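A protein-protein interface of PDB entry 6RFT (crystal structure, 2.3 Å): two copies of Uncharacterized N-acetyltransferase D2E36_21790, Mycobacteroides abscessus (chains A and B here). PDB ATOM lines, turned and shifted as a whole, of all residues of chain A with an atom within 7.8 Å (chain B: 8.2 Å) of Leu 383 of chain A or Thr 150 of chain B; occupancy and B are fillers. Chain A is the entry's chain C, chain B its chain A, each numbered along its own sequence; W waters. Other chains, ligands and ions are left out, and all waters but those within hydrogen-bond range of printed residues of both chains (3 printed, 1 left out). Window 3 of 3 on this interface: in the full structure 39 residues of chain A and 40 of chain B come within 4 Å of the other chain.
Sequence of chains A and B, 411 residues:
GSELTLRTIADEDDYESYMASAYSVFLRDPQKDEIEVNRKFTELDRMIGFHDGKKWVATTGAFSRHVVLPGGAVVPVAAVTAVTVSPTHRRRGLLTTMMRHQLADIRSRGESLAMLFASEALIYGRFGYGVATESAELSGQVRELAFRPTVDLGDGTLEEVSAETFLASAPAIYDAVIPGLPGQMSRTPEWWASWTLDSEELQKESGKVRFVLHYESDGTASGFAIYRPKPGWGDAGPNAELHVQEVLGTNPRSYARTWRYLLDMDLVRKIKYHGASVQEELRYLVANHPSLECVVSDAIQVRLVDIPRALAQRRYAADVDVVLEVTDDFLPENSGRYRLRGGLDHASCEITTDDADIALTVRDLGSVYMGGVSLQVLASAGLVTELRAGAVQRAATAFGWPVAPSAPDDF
Val 377 of chain A touches Tyr 284 of chain B. O of Ser 380 of chain A touches CG of Pro 252 of chain B, at 3.5 Å. OE2 of Glu 281 of chain B touches CB of Ser 380 of chain A, at 3.5 Å. CB of Ala 381 of chain A touches CG of Glu 281 of chain B, 3.8 Å away. Leu 285 of chain B touches Ala 381 of chain A. Gly 382 of chain A touches Pro 252 of chain B. Leu 383 of chain A touches Arg 148 of chain B (CD1 to NH1, 3.5 Å). CD2 of Leu 383 of chain A touches OG1 of Thr 150 of chain B, at 3.9 Å. Val 151 of chain B touches Leu 383 of chain A. Leu 383 of chain A touches Tyr 284 of chain B (CD1 to O, 3.5 Å).
Water W2 lies within hydrogen-bond range of NH2 of Arg 148 of chain B and OG1 of Thr 361 of chain A. Water W3 lies within hydrogen-bond range of the backbone carbonyl oxygen of Leu 383 of chain A (2.9 Å) and the side-chain hydroxyl of Thr 150 of chain B (3.3 Å). Water W1 lies within hydrogen-bond range of the backbone carbonyl oxygen (O) of Val 286 of chain B (3.0 Å), a ring nitrogen (NE2) of His 289 of chain B (3.2 Å) and the guanidinium group (NH2) of Arg 363 of chain A (3.4 Å).
No position is printed for both chains. Of the 13 pairs that touch across the chains among the printed residues, none has its exchanged pair printed and touching as well.
Leu 383 of chain A touches just these residues of chain B: Arg 148 (3.5 Å), Thr 150 (3.9 Å), Val 151 (3.9 Å) and Tyr 284 (3.5 Å). No residue of chain A comes within 4 Å of Pro 149 of chain B. Printed residues of chain A within 4 Å of Arg 148 of chain B: Arg 363, Asp 364 and Leu 383. Of the printed residues of chain A, Pro 252 of chain B touches Ser 380 (3.5 Å), Ala 381 (3.6 Å) and Gly 382 (3.7 Å). Of the printed residues of chain B, Arg 363 of chain A touches Arg 148 (3.5 Å). Printed residues of chain B within 4 Å of Ala 381 of chain A: Pro 252, Glu 281 and Leu 285. Ala 379 of chain A touches none of the printed residues of chain B. Glu 386 of chain A touches none of the printed residues of chain B. The nearest residue of chain B that does not touch Leu 383 of chain A is Leu 285 of chain B (4.8 Å). The nearest printed residue of chain A that does not touch Glu 281 of chain B is Val 377 of chain A (4.1 Å).
NH1 of Arg 148 of chain B is in salt-bridge range of OD1 of Asp 364 of chain A, 2.8 Å away.
Hydrophobic or aromatic side chains of chain A within 4 Å of the printed part of chain B: Val 377, Ala 381 and Leu 383. Along chain A the printed residues that touch a printed residue of chain B span positions 363 to 383. Printed residues of chain B that touch a printed residue of chain A: Arg 148, Thr 150, Val 151, Pro 252, Glu 281, Tyr 284 and Leu 285. Hydrophobic or aromatic side chains of chain B within 4 Å of the printed part of chain A: Val 151, Pro 252, Tyr 284 and Leu 285. Among the printed residues, Asp or Glu carboxylates within 4 Å of a Lys or Arg side-chain nitrogen of the other chain: Asp 364 of chain A with Arg 148 of chain B.
N of Arg 148 of chain B is in hydrogen-bond range of O of Leu 285 of chain B (2.8 Å). The side-chain carboxylate (OD2) of Asp 364 of chain A is in hydrogen-bond range of the side-chain hydroxyl (OG1) of Thr 361 of chain A (3.0 Å). O of Leu 378 of chain A is in hydrogen-bond range of N of Leu 383 of chain A, 3.1 Å away.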
ATOM      1  N   ASP A 329      26.721  14.054   3.698  1.00  0.00           N
ATOM      2  CA  ASP A 329      27.392  14.767   2.614  1.00  0.00           C
ATOM      3  C   ASP A 329      28.905  14.590   2.668  1.00  0.00           C
ATOM      4  O   ASP A 329      29.544  14.367   1.633  1.00  0.00           O
ATOM      5  CB  ASP A 329      27.028  16.251   2.669  1.00  0.00           C
ATOM      6  CG  ASP A 329      25.597  16.515   2.252  1.00  0.00           C
ATOM      7  OD1 ASP A 329      25.120  15.853   1.306  1.00  0.00           O
ATOM      8  OD2 ASP A 329      24.947  17.382   2.873  1.00  0.00           O
ATOM      9  N   ALA A 359      13.153  12.257   6.139  1.00  0.00           N
ATOM     10  CA  ALA A 359      14.379  12.586   5.426  1.00  0.00           C
ATOM     11  C   ALA A 359      15.169  13.601   6.238  1.00  0.00           C
ATOM     12  O   ALA A 359      14.621  14.626   6.660  1.00  0.00           O
ATOM     13  CB  ALA A 359      14.075  13.140   4.032  1.00  0.00           C
ATOM     14  N   LEU A 360      16.450  13.315   6.459  1.00  0.00           N
ATOM     15  CA  LEU A 360      17.285  14.185   7.275  1.00  0.00           C
ATOM     16  C   LEU A 360      18.747  13.917   6.956  1.00  0.00           C
ATOM     17  O   LEU A 360      19.102  12.875   6.399  1.00  0.00           O
ATOM     18  CB  LEU A 360      17.018  13.981   8.773  1.00  0.00           C
ATOM     19  CG  LEU A 360      17.627  12.760   9.473  1.00  0.00           C
ATOM     20  CD1 LEU A 360      17.408  12.857  10.973  1.00  0.00           C
ATOM     21  CD2 LEU A 360      17.059  11.449   8.945  1.00  0.00           C
ATOM     22  N   THR A 361      19.590  14.879   7.320  1.00  0.00           N
ATOM     23  CA  THR A 361      21.030  14.761   7.154  1.00  0.00           C
ATOM     24  C   THR A 361      21.651  14.090   8.376  1.00  0.00           C
ATOM     25  O   THR A 361      21.033  13.980   9.437  1.00  0.00           O
ATOM     26  CB  THR A 361      21.669  16.132   6.932  1.00  0.00           C
ATOM     27  OG1 THR A 361      21.454  16.954   8.087  1.00  0.00           O
ATOM     28  CG2 THR A 361      21.064  16.812   5.712  1.00  0.00           C
ATOM     29  N   ARG A 363      24.070  15.169  10.182  1.00  0.00           N
ATOM     30  CA  ARG A 363      24.322  16.119  11.262  1.00  0.00           C
ATOM     31  C   ARG A 363      23.068  16.355  12.098  1.00  0.00           C
ATOM     32  O   ARG A 363      23.150  16.486  13.324  1.00  0.00           O
ATOM     33  CB  ARG A 363      24.861  17.438  10.699  1.00  0.00           C
ATOM     34  CG  ARG A 363      23.881  18.227   9.839  1.00  0.00           C
ATOM     35  CD  ARG A 363      24.392  19.633   9.546  1.00  0.00           C
ATOM     36  NE  ARG A 363      24.347  20.495  10.725  1.00  0.00           N
ATOM     37  CZ  ARG A 363      24.715  21.773  10.732  1.00  0.00           C
ATOM     38  NH1 ARG A 363      25.160  22.344   9.621  1.00  0.00           N
ATOM     39  NH2 ARG A 363      24.639  22.481  11.851  1.00  0.00           N
ATOM     40  N   ASP A 364      21.899  16.410  11.454  1.00  0.00           N
ATOM     41  CA  ASP A 364      20.656  16.579  12.202  1.00  0.00           C
ATOM     42  C   ASP A 364      20.304  15.315  12.975  1.00  0.00           C
ATOM     43  O   ASP A 364      19.760  15.391  14.083  1.00  0.00           O
ATOM     44  CB  ASP A 364      19.523  16.972  11.256  1.00  0.00           C
ATOM     45  CG  ASP A 364      19.673  18.384  10.724  1.00  0.00           C
ATOM     46  OD1 ASP A 364      20.059  19.277  11.507  1.00  0.00           O
ATOM     47  OD2 ASP A 364      19.405  18.600   9.524  1.00  0.00           O
ATOM     48  N   LEU A 375      13.347  16.248  17.381  1.00  0.00           N
ATOM     49  CA  LEU A 375      13.223  16.011  15.947  1.00  0.00           C
ATOM     50  C   LEU A 375      12.015  16.734  15.363  1.00  0.00           C
ATOM     51  O   LEU A 375      12.014  17.077  14.176  1.00  0.00           O
ATOM     52  CB  LEU A 375      13.129  14.510  15.671  1.00  0.00           C
ATOM     53  CG  LEU A 375      13.135  14.061  14.207  1.00  0.00           C
ATOM     54  CD1 LEU A 375      14.451  14.418  13.535  1.00  0.00           C
ATOM     55  CD2 LEU A 375      12.861  12.568  14.102  1.00  0.00           C
ATOM     56  N   VAL A 377      10.942  19.788  16.289  1.00  0.00           N
ATOM     57  CA  VAL A 377      11.327  21.180  16.073  1.00  0.00           C
ATOM     58  C   VAL A 377      12.173  21.310  14.813  1.00  0.00           C
ATOM     59  O   VAL A 377      11.991  22.242  14.020  1.00  0.00           O
ATOM     60  CB  VAL A 377      12.061  21.731  17.310  1.00  0.00           C
ATOM     61  CG1 VAL A 377      12.478  23.174  17.082  1.00  0.00           C
ATOM     62  CG2 VAL A 377      11.176  21.620  18.542  1.00  0.00           C
ATOM     63  N   LEU A 378      13.109  20.380  14.608  1.00  0.00           N
ATOM     64  CA  LEU A 378      13.921  20.406  13.396  1.00  0.00           C
ATOM     65  C   LEU A 378      13.065  20.233  12.147  1.00  0.00           C
ATOM     66  O   LEU A 378      13.380  20.804  11.096  1.00  0.00           O
ATOM     67  CB  LEU A 378      14.994  19.318  13.457  1.00  0.00           C
ATOM     68  CG  LEU A 378      16.031  19.436  14.577  1.00  0.00           C
ATOM     69  CD1 LEU A 378      17.095  18.359  14.435  1.00  0.00           C
ATOM     70  CD2 LEU A 378      16.663  20.818  14.582  1.00  0.00           C
ATOM     71  N   ALA A 379      11.987  19.453  12.241  1.00  0.00           N
ATOM     72  CA  ALA A 379      11.092  19.282  11.101  1.00  0.00           C
ATOM     73  C   ALA A 379      10.232  20.521  10.885  1.00  0.00           C
ATOM     74  O   ALA A 379      10.070  20.987   9.750  1.00  0.00           O
ATOM     75  CB  ALA A 379      10.217  18.045  11.302  1.00  0.00           C
ATOM     76  N   SER A 380       9.665  21.067  11.966  1.00  0.00           N
ATOM     77  CA  SER A 380       8.864  22.283  11.853  1.00  0.00           C
ATOM     78  C   SER A 380       9.697  23.462  11.368  1.00  0.00           C
ATOM     79  O   SER A 380       9.155  24.408  10.785  1.00  0.00           O
ATOM     80  CB  SER A 380       8.215  22.609  13.198  1.00  0.00           C
ATOM     81  OG  SER A 380       7.371  21.553  13.624  1.00  0.00           O
ATOM     82  N   ALA A 381      11.009  23.428  11.601  1.00  0.00           N
ATOM     83  CA  ALA A 381      11.900  24.487  11.148  1.00  0.00           C
ATOM     84  C   ALA A 381      12.278  24.361   9.679  1.00  0.00           C
ATOM     85  O   ALA A 381      12.881  25.289   9.130  1.00  0.00           O
ATOM     86  CB  ALA A 381      13.168  24.501  12.003  1.00  0.00           C
ATOM     87  N   GLY A 382      11.942  23.246   9.032  1.00  0.00           N
ATOM     88  CA  GLY A 382      12.283  23.029   7.642  1.00  0.00           C
ATOM     89  C   GLY A 382      13.597  22.318   7.403  1.00  0.00           C
ATOM     90  O   GLY A 382      13.934  22.051   6.242  1.00  0.00           O
ATOM     91  N   LEU A 383      14.347  21.996   8.458  1.00  0.00           N
ATOM     92  CA  LEU A 383      15.618  21.302   8.289  1.00  0.00           C
ATOM     93  C   LEU A 383      15.428  19.807   8.069  1.00  0.00           C
ATOM     94  O   LEU A 383      16.263  19.170   7.418  1.00  0.00           O
ATOM     95  CB  LEU A 383      16.512  21.545   9.506  1.00  0.00           C
ATOM     96  CG  LEU A 383      16.846  23.006   9.807  1.00  0.00           C
ATOM     97  CD1 LEU A 383      17.410  23.157  11.212  1.00  0.00           C
ATOM     98  CD2 LEU A 383      17.818  23.552   8.774  1.00  0.00           C
ATOM     99  N   VAL A 384      14.349  19.237   8.598  1.00  0.00           N
ATOM    100  CA  VAL A 384      14.040  17.820   8.456  1.00  0.00           C
ATOM    101  C   VAL A 384      12.690  17.694   7.762  1.00  0.00           C
ATOM    102  O   VAL A 384      11.764  18.461   8.045  1.00  0.00           O
ATOM    103  CB  VAL A 384      14.035  17.109   9.827  1.00  0.00           C
ATOM    104  CG1 VAL A 384      13.591  15.669   9.686  1.00  0.00           C
ATOM    105  CG2 VAL A 384      15.415  17.181  10.461  1.00  0.00           C
ATOM    106  N   THR A 385      12.581  16.728   6.855  1.00  0.00           N
ATOM    107  CA  THR A 385      11.397  16.554   6.024  1.00  0.00           C
ATOM    108  C   THR A 385      10.642  15.297   6.435  1.00  0.00           C
ATOM    109  O   THR A 385      11.226  14.209   6.502  1.00  0.00           O
ATOM    110  CB  THR A 385      11.777  16.473   4.544  1.00  0.00           C
ATOM    111  OG1 THR A 385      12.508  17.649   4.170  1.00  0.00           O
ATOM    112  CG2 THR A 385      10.532  16.360   3.678  1.00  0.00           C
ATOM    113  N   GLU A 386       9.348  15.451   6.710  1.00  0.00           N
ATOM    114  CA  GLU A 386       8.470  14.324   6.992  1.00  0.00           C
ATOM    115  C   GLU A 386       7.909  13.774   5.688  1.00  0.00           C
ATOM    116  O   GLU A 386       7.368  14.527   4.871  1.00  0.00           O
ATOM    117  CB  GLU A 386       7.325  14.740   7.916  1.00  0.00           C
ATOM    118  CG  GLU A 386       6.460  13.575   8.377  1.00  0.00           C
ATOM    119  CD  GLU A 386       5.332  14.008   9.293  1.00  0.00           C
ATOM    120  OE1 GLU A 386       4.596  14.947   8.928  1.00  0.00           O
ATOM    121  OE2 GLU A 386       5.183  13.408  10.379  1.00  0.00           O
ATOM    122  N   PHE B 147      21.779  32.214   8.722  1.00  0.00           N
ATOM    123  CA  PHE B 147      21.120  30.924   8.835  1.00  0.00           C
ATOM    124  C   PHE B 147      21.989  29.820   8.247  1.00  0.00           C
ATOM    125  O   PHE B 147      22.959  30.072   7.528  1.00  0.00           O
ATOM    126  CB  PHE B 147      19.759  30.951   8.138  1.00  0.00           C
ATOM    127  CG  PHE B 147      18.726  31.768   8.859  1.00  0.00           C
ATOM    128  CD1 PHE B 147      18.904  32.117  10.188  1.00  0.00           C
ATOM    129  CD2 PHE B 147      17.578  32.187   8.208  1.00  0.00           C
ATOM    130  CE1 PHE B 147      17.956  32.870  10.853  1.00  0.00           C
ATOM    131  CE2 PHE B 147      16.626  32.939   8.868  1.00  0.00           C
ATOM    132  CZ  PHE B 147      16.815  33.281  10.193  1.00  0.00           C
ATOM    133  N   ARG B 148      21.633  28.580   8.579  1.00  0.00           N
ATOM    134  CA  ARG B 148      22.295  27.439   7.973  1.00  0.00           C
ATOM    135  C   ARG B 148      22.076  27.470   6.461  1.00  0.00           C
ATOM    136  O   ARG B 148      21.046  27.955   5.985  1.00  0.00           O
ATOM    137  CB  ARG B 148      21.762  26.134   8.565  1.00  0.00           C
ATOM    138  CG  ARG B 148      22.347  25.790   9.928  1.00  0.00           C
ATOM    139  CD  ARG B 148      21.650  24.590  10.556  1.00  0.00           C
ATOM    140  NE  ARG B 148      21.668  23.415   9.689  1.00  0.00           N
ATOM    141  CZ  ARG B 148      21.216  22.216  10.047  1.00  0.00           C
ATOM    142  NH1 ARG B 148      20.713  22.031  11.261  1.00  0.00           N
ATOM    143  NH2 ARG B 148      21.269  21.202   9.194  1.00  0.00           N
ATOM    144  N   PRO B 149      23.035  26.967   5.679  1.00  0.00           N
ATOM    145  CA  PRO B 149      22.929  27.098   4.216  1.00  0.00           C
ATOM    146  C   PRO B 149      21.755  26.352   3.604  1.00  0.00           C
ATOM    147  O   PRO B 149      21.352  26.686   2.483  1.00  0.00           O
ATOM    148  CB  PRO B 149      24.270  26.543   3.715  1.00  0.00           C
ATOM    149  CG  PRO B 149      24.758  25.666   4.821  1.00  0.00           C
ATOM    150  CD  PRO B 149      24.289  26.310   6.088  1.00  0.00           C
ATOM    151  N   THR B 150      21.188  25.364   4.291  1.00  0.00           N
ATOM    152  CA  THR B 150      20.086  24.585   3.745  1.00  0.00           C
ATOM    153  C   THR B 150      18.717  25.159   4.091  1.00  0.00           C
ATOM    154  O   THR B 150      17.700  24.525   3.789  1.00  0.00           O
ATOM    155  CB  THR B 150      20.173  23.134   4.229  1.00  0.00           C
ATOM    156  OG1 THR B 150      20.138  23.101   5.661  1.00  0.00           O
ATOM    157  CG2 THR B 150      21.462  22.488   3.742  1.00  0.00           C
ATOM    158  N   VAL B 151      18.663  26.335   4.711  1.00  0.00           N
ATOM    159  CA  VAL B 151      17.392  26.947   5.086  1.00  0.00           C
ATOM    160  C   VAL B 151      16.797  27.636   3.863  1.00  0.00           C
ATOM    161  O   VAL B 151      17.413  28.537   3.284  1.00  0.00           O
ATOM    162  CB  VAL B 151      17.572  27.935   6.247  1.00  0.00           C
ATOM    163  CG1 VAL B 151      16.264  28.654   6.535  1.00  0.00           C
ATOM    164  CG2 VAL B 151      18.071  27.206   7.486  1.00  0.00           C
ATOM    165  N   ASP B 152      15.597  27.214   3.471  1.00  0.00           N
ATOM    166  CA  ASP B 152      14.918  27.766   2.306  1.00  0.00           C
ATOM    167  C   ASP B 152      14.068  28.958   2.732  1.00  0.00           C
ATOM    168  O   ASP B 152      13.168  28.819   3.569  1.00  0.00           O
ATOM    169  CB  ASP B 152      14.056  26.700   1.631  1.00  0.00           C
ATOM    170  CG  ASP B 152      13.470  27.170   0.311  1.00  0.00           C
ATOM    171  OD1 ASP B 152      13.840  28.270  -0.153  1.00  0.00           O
ATOM    172  OD2 ASP B 152      12.638  26.437  -0.263  1.00  0.00           O
ATOM    173  N   LEU B 153      14.351  30.125   2.155  1.00  0.00           N
ATOM    174  CA  LEU B 153      13.606  31.341   2.456  1.00  0.00           C
ATOM    175  C   LEU B 153      12.375  31.521   1.577  1.00  0.00           C
ATOM    176  O   LEU B 153      11.543  32.384   1.875  1.00  0.00           O
ATOM    177  CB  LEU B 153      14.514  32.568   2.314  1.00  0.00           C
ATOM    178  CG  LEU B 153      15.759  32.608   3.202  1.00  0.00           C
ATOM    179  CD1 LEU B 153      16.569  33.868   2.935  1.00  0.00           C
ATOM    180  CD2 LEU B 153      15.376  32.514   4.673  1.00  0.00           C
ATOM    181  N   PRO B 252       7.690  26.709   7.018  1.00  0.00           N
ATOM    182  CA  PRO B 252       9.065  27.103   7.375  1.00  0.00           C
ATOM    183  C   PRO B 252       9.612  28.253   6.547  1.00  0.00           C
ATOM    184  O   PRO B 252      10.434  29.026   7.055  1.00  0.00           O
ATOM    185  CB  PRO B 252       9.870  25.815   7.146  1.00  0.00           C
ATOM    186  CG  PRO B 252       8.873  24.717   7.262  1.00  0.00           C
ATOM    187  CD  PRO B 252       7.592  25.269   6.717  1.00  0.00           C
ATOM    188  N   GLU B 281      12.120  27.853  16.833  1.00  0.00           N
ATOM    189  CA  GLU B 281      12.736  27.386  15.593  1.00  0.00           C
ATOM    190  C   GLU B 281      13.924  28.251  15.186  1.00  0.00           C
ATOM    191  O   GLU B 281      14.870  27.749  14.567  1.00  0.00           O
ATOM    192  CB  GLU B 281      11.702  27.355  14.469  1.00  0.00           C
ATOM    193  CG  GLU B 281      10.818  26.118  14.457  1.00  0.00           C
ATOM    194  CD  GLU B 281       9.504  26.332  15.182  1.00  0.00           C
ATOM    195  OE1 GLU B 281       9.475  27.119  16.153  1.00  0.00           O
ATOM    196  OE2 GLU B 281       8.497  25.713  14.779  1.00  0.00           O
ATOM    197  N   LEU B 282      13.889  29.548  15.511  1.00  0.00           N
ATOM    198  CA  LEU B 282      14.997  30.436  15.170  1.00  0.00           C
ATOM    199  C   LEU B 282      16.317  29.948  15.754  1.00  0.00           C
ATOM    200  O   LEU B 282      17.370  30.122  15.131  1.00  0.00           O
ATOM    201  CB  LEU B 282      14.695  31.857  15.649  1.00  0.00           C
ATOM    202  CG  LEU B 282      15.774  32.910  15.380  1.00  0.00           C
ATOM    203  CD1 LEU B 282      15.930  33.154  13.886  1.00  0.00           C
ATOM    204  CD2 LEU B 282      15.452  34.203  16.106  1.00  0.00           C
ATOM    205  N   ARG B 283      16.282  29.339  16.943  1.00  0.00           N
ATOM    206  CA  ARG B 283      17.512  28.885  17.587  1.00  0.00           C
ATOM    207  C   ARG B 283      18.248  27.857  16.739  1.00  0.00           C
ATOM    208  O   ARG B 283      19.483  27.805  16.757  1.00  0.00           O
ATOM    209  CB  ARG B 283      17.197  28.304  18.967  1.00  0.00           C
ATOM    210  CG  ARG B 283      16.397  29.235  19.865  1.00  0.00           C
ATOM    211  CD  ARG B 283      16.233  28.667  21.268  1.00  0.00           C
ATOM    212  NE  ARG B 283      17.510  28.520  21.960  1.00  0.00           N
ATOM    213  CZ  ARG B 283      17.970  27.370  22.444  1.00  0.00           C
ATOM    214  NH1 ARG B 283      17.254  26.261  22.319  1.00  0.00           N
ATOM    215  NH2 ARG B 283      19.144  27.330  23.060  1.00  0.00           N
ATOM    216  N   TYR B 284      17.513  27.035  15.990  1.00  0.00           N
ATOM    217  CA  TYR B 284      18.105  25.999  15.157  1.00  0.00           C
ATOM    218  C   TYR B 284      18.297  26.432  13.710  1.00  0.00           C
ATOM    219  O   TYR B 284      18.995  25.742  12.961  1.00  0.00           O
ATOM    220  CB  TYR B 284      17.246  24.732  15.223  1.00  0.00           C
ATOM    221  CG  TYR B 284      16.939  24.324  16.645  1.00  0.00           C
ATOM    222  CD1 TYR B 284      17.845  23.574  17.383  1.00  0.00           C
ATOM    223  CD2 TYR B 284      15.760  24.720  17.263  1.00  0.00           C
ATOM    224  CE1 TYR B 284      17.577  23.211  18.688  1.00  0.00           C
ATOM    225  CE2 TYR B 284      15.484  24.362  18.569  1.00  0.00           C
ATOM    226  CZ  TYR B 284      16.395  23.608  19.276  1.00  0.00           C
ATOM    227  OH  TYR B 284      16.123  23.250  20.576  1.00  0.00           O
ATOM    228  N   LEU B 285      17.699  27.555  13.303  1.00  0.00           N
ATOM    229  CA  LEU B 285      17.990  28.111  11.985  1.00  0.00           C
ATOM    230  C   LEU B 285      19.360  28.772  11.951  1.00  0.00           C
ATOM    231  O   LEU B 285      20.032  28.749  10.914  1.00  0.00           O
ATOM    232  CB  LEU B 285      16.914  29.120  11.583  1.00  0.00           C
ATOM    233  CG  LEU B 285      15.717  28.636  10.760  1.00  0.00           C
ATOM    234  CD1 LEU B 285      15.158  27.344  11.312  1.00  0.00           C
ATOM    235  CD2 LEU B 285      14.638  29.708  10.713  1.00  0.00           C
ATOM    236  N   VAL B 286      19.786  29.360  13.069  1.00  0.00           N
ATOM    237  CA  VAL B 286      21.043  30.096  13.111  1.00  0.00           C
ATOM    238  C   VAL B 286      22.202  29.134  12.896  1.00  0.00           C
ATOM    239  O   VAL B 286      22.256  28.054  13.499  1.00  0.00           O
ATOM    240  CB  VAL B 286      21.173  30.847  14.445  1.00  0.00           C
ATOM    241  CG1 VAL B 286      22.531  31.506  14.561  1.00  0.00           C
ATOM    242  CG2 VAL B 286      20.067  31.880  14.582  1.00  0.00           C
ATOM    243  N   HIS B 289      24.919  28.733  16.707  1.00  0.00           N
ATOM    244  CA  HIS B 289      24.035  28.742  17.873  1.00  0.00           C
ATOM    245  C   HIS B 289      24.459  29.700  18.983  1.00  0.00           C
ATOM    246  O   HIS B 289      23.587  30.412  19.508  1.00  0.00           O
ATOM    247  CB  HIS B 289      23.902  27.314  18.422  1.00  0.00           C
ATOM    248  CG  HIS B 289      23.084  26.406  17.556  1.00  0.00           C
ATOM    249  ND1 HIS B 289      22.785  25.110  17.916  1.00  0.00           N
ATOM    250  CD2 HIS B 289      22.498  26.608  16.353  1.00  0.00           C
ATOM    251  CE1 HIS B 289      22.052  24.550  16.970  1.00  0.00           C
ATOM    252  NE2 HIS B 289      21.863  25.438  16.010  1.00  0.00           N
HETATM  253  O   HOH W   1      23.435  25.327  13.262  1.00  0.00           O
HETATM  254  O   HOH W   2      21.712  20.085   6.777  1.00  0.00           O
HETATM  255  O   HOH W   3      18.567  20.272   5.985  1.00  0.00           O
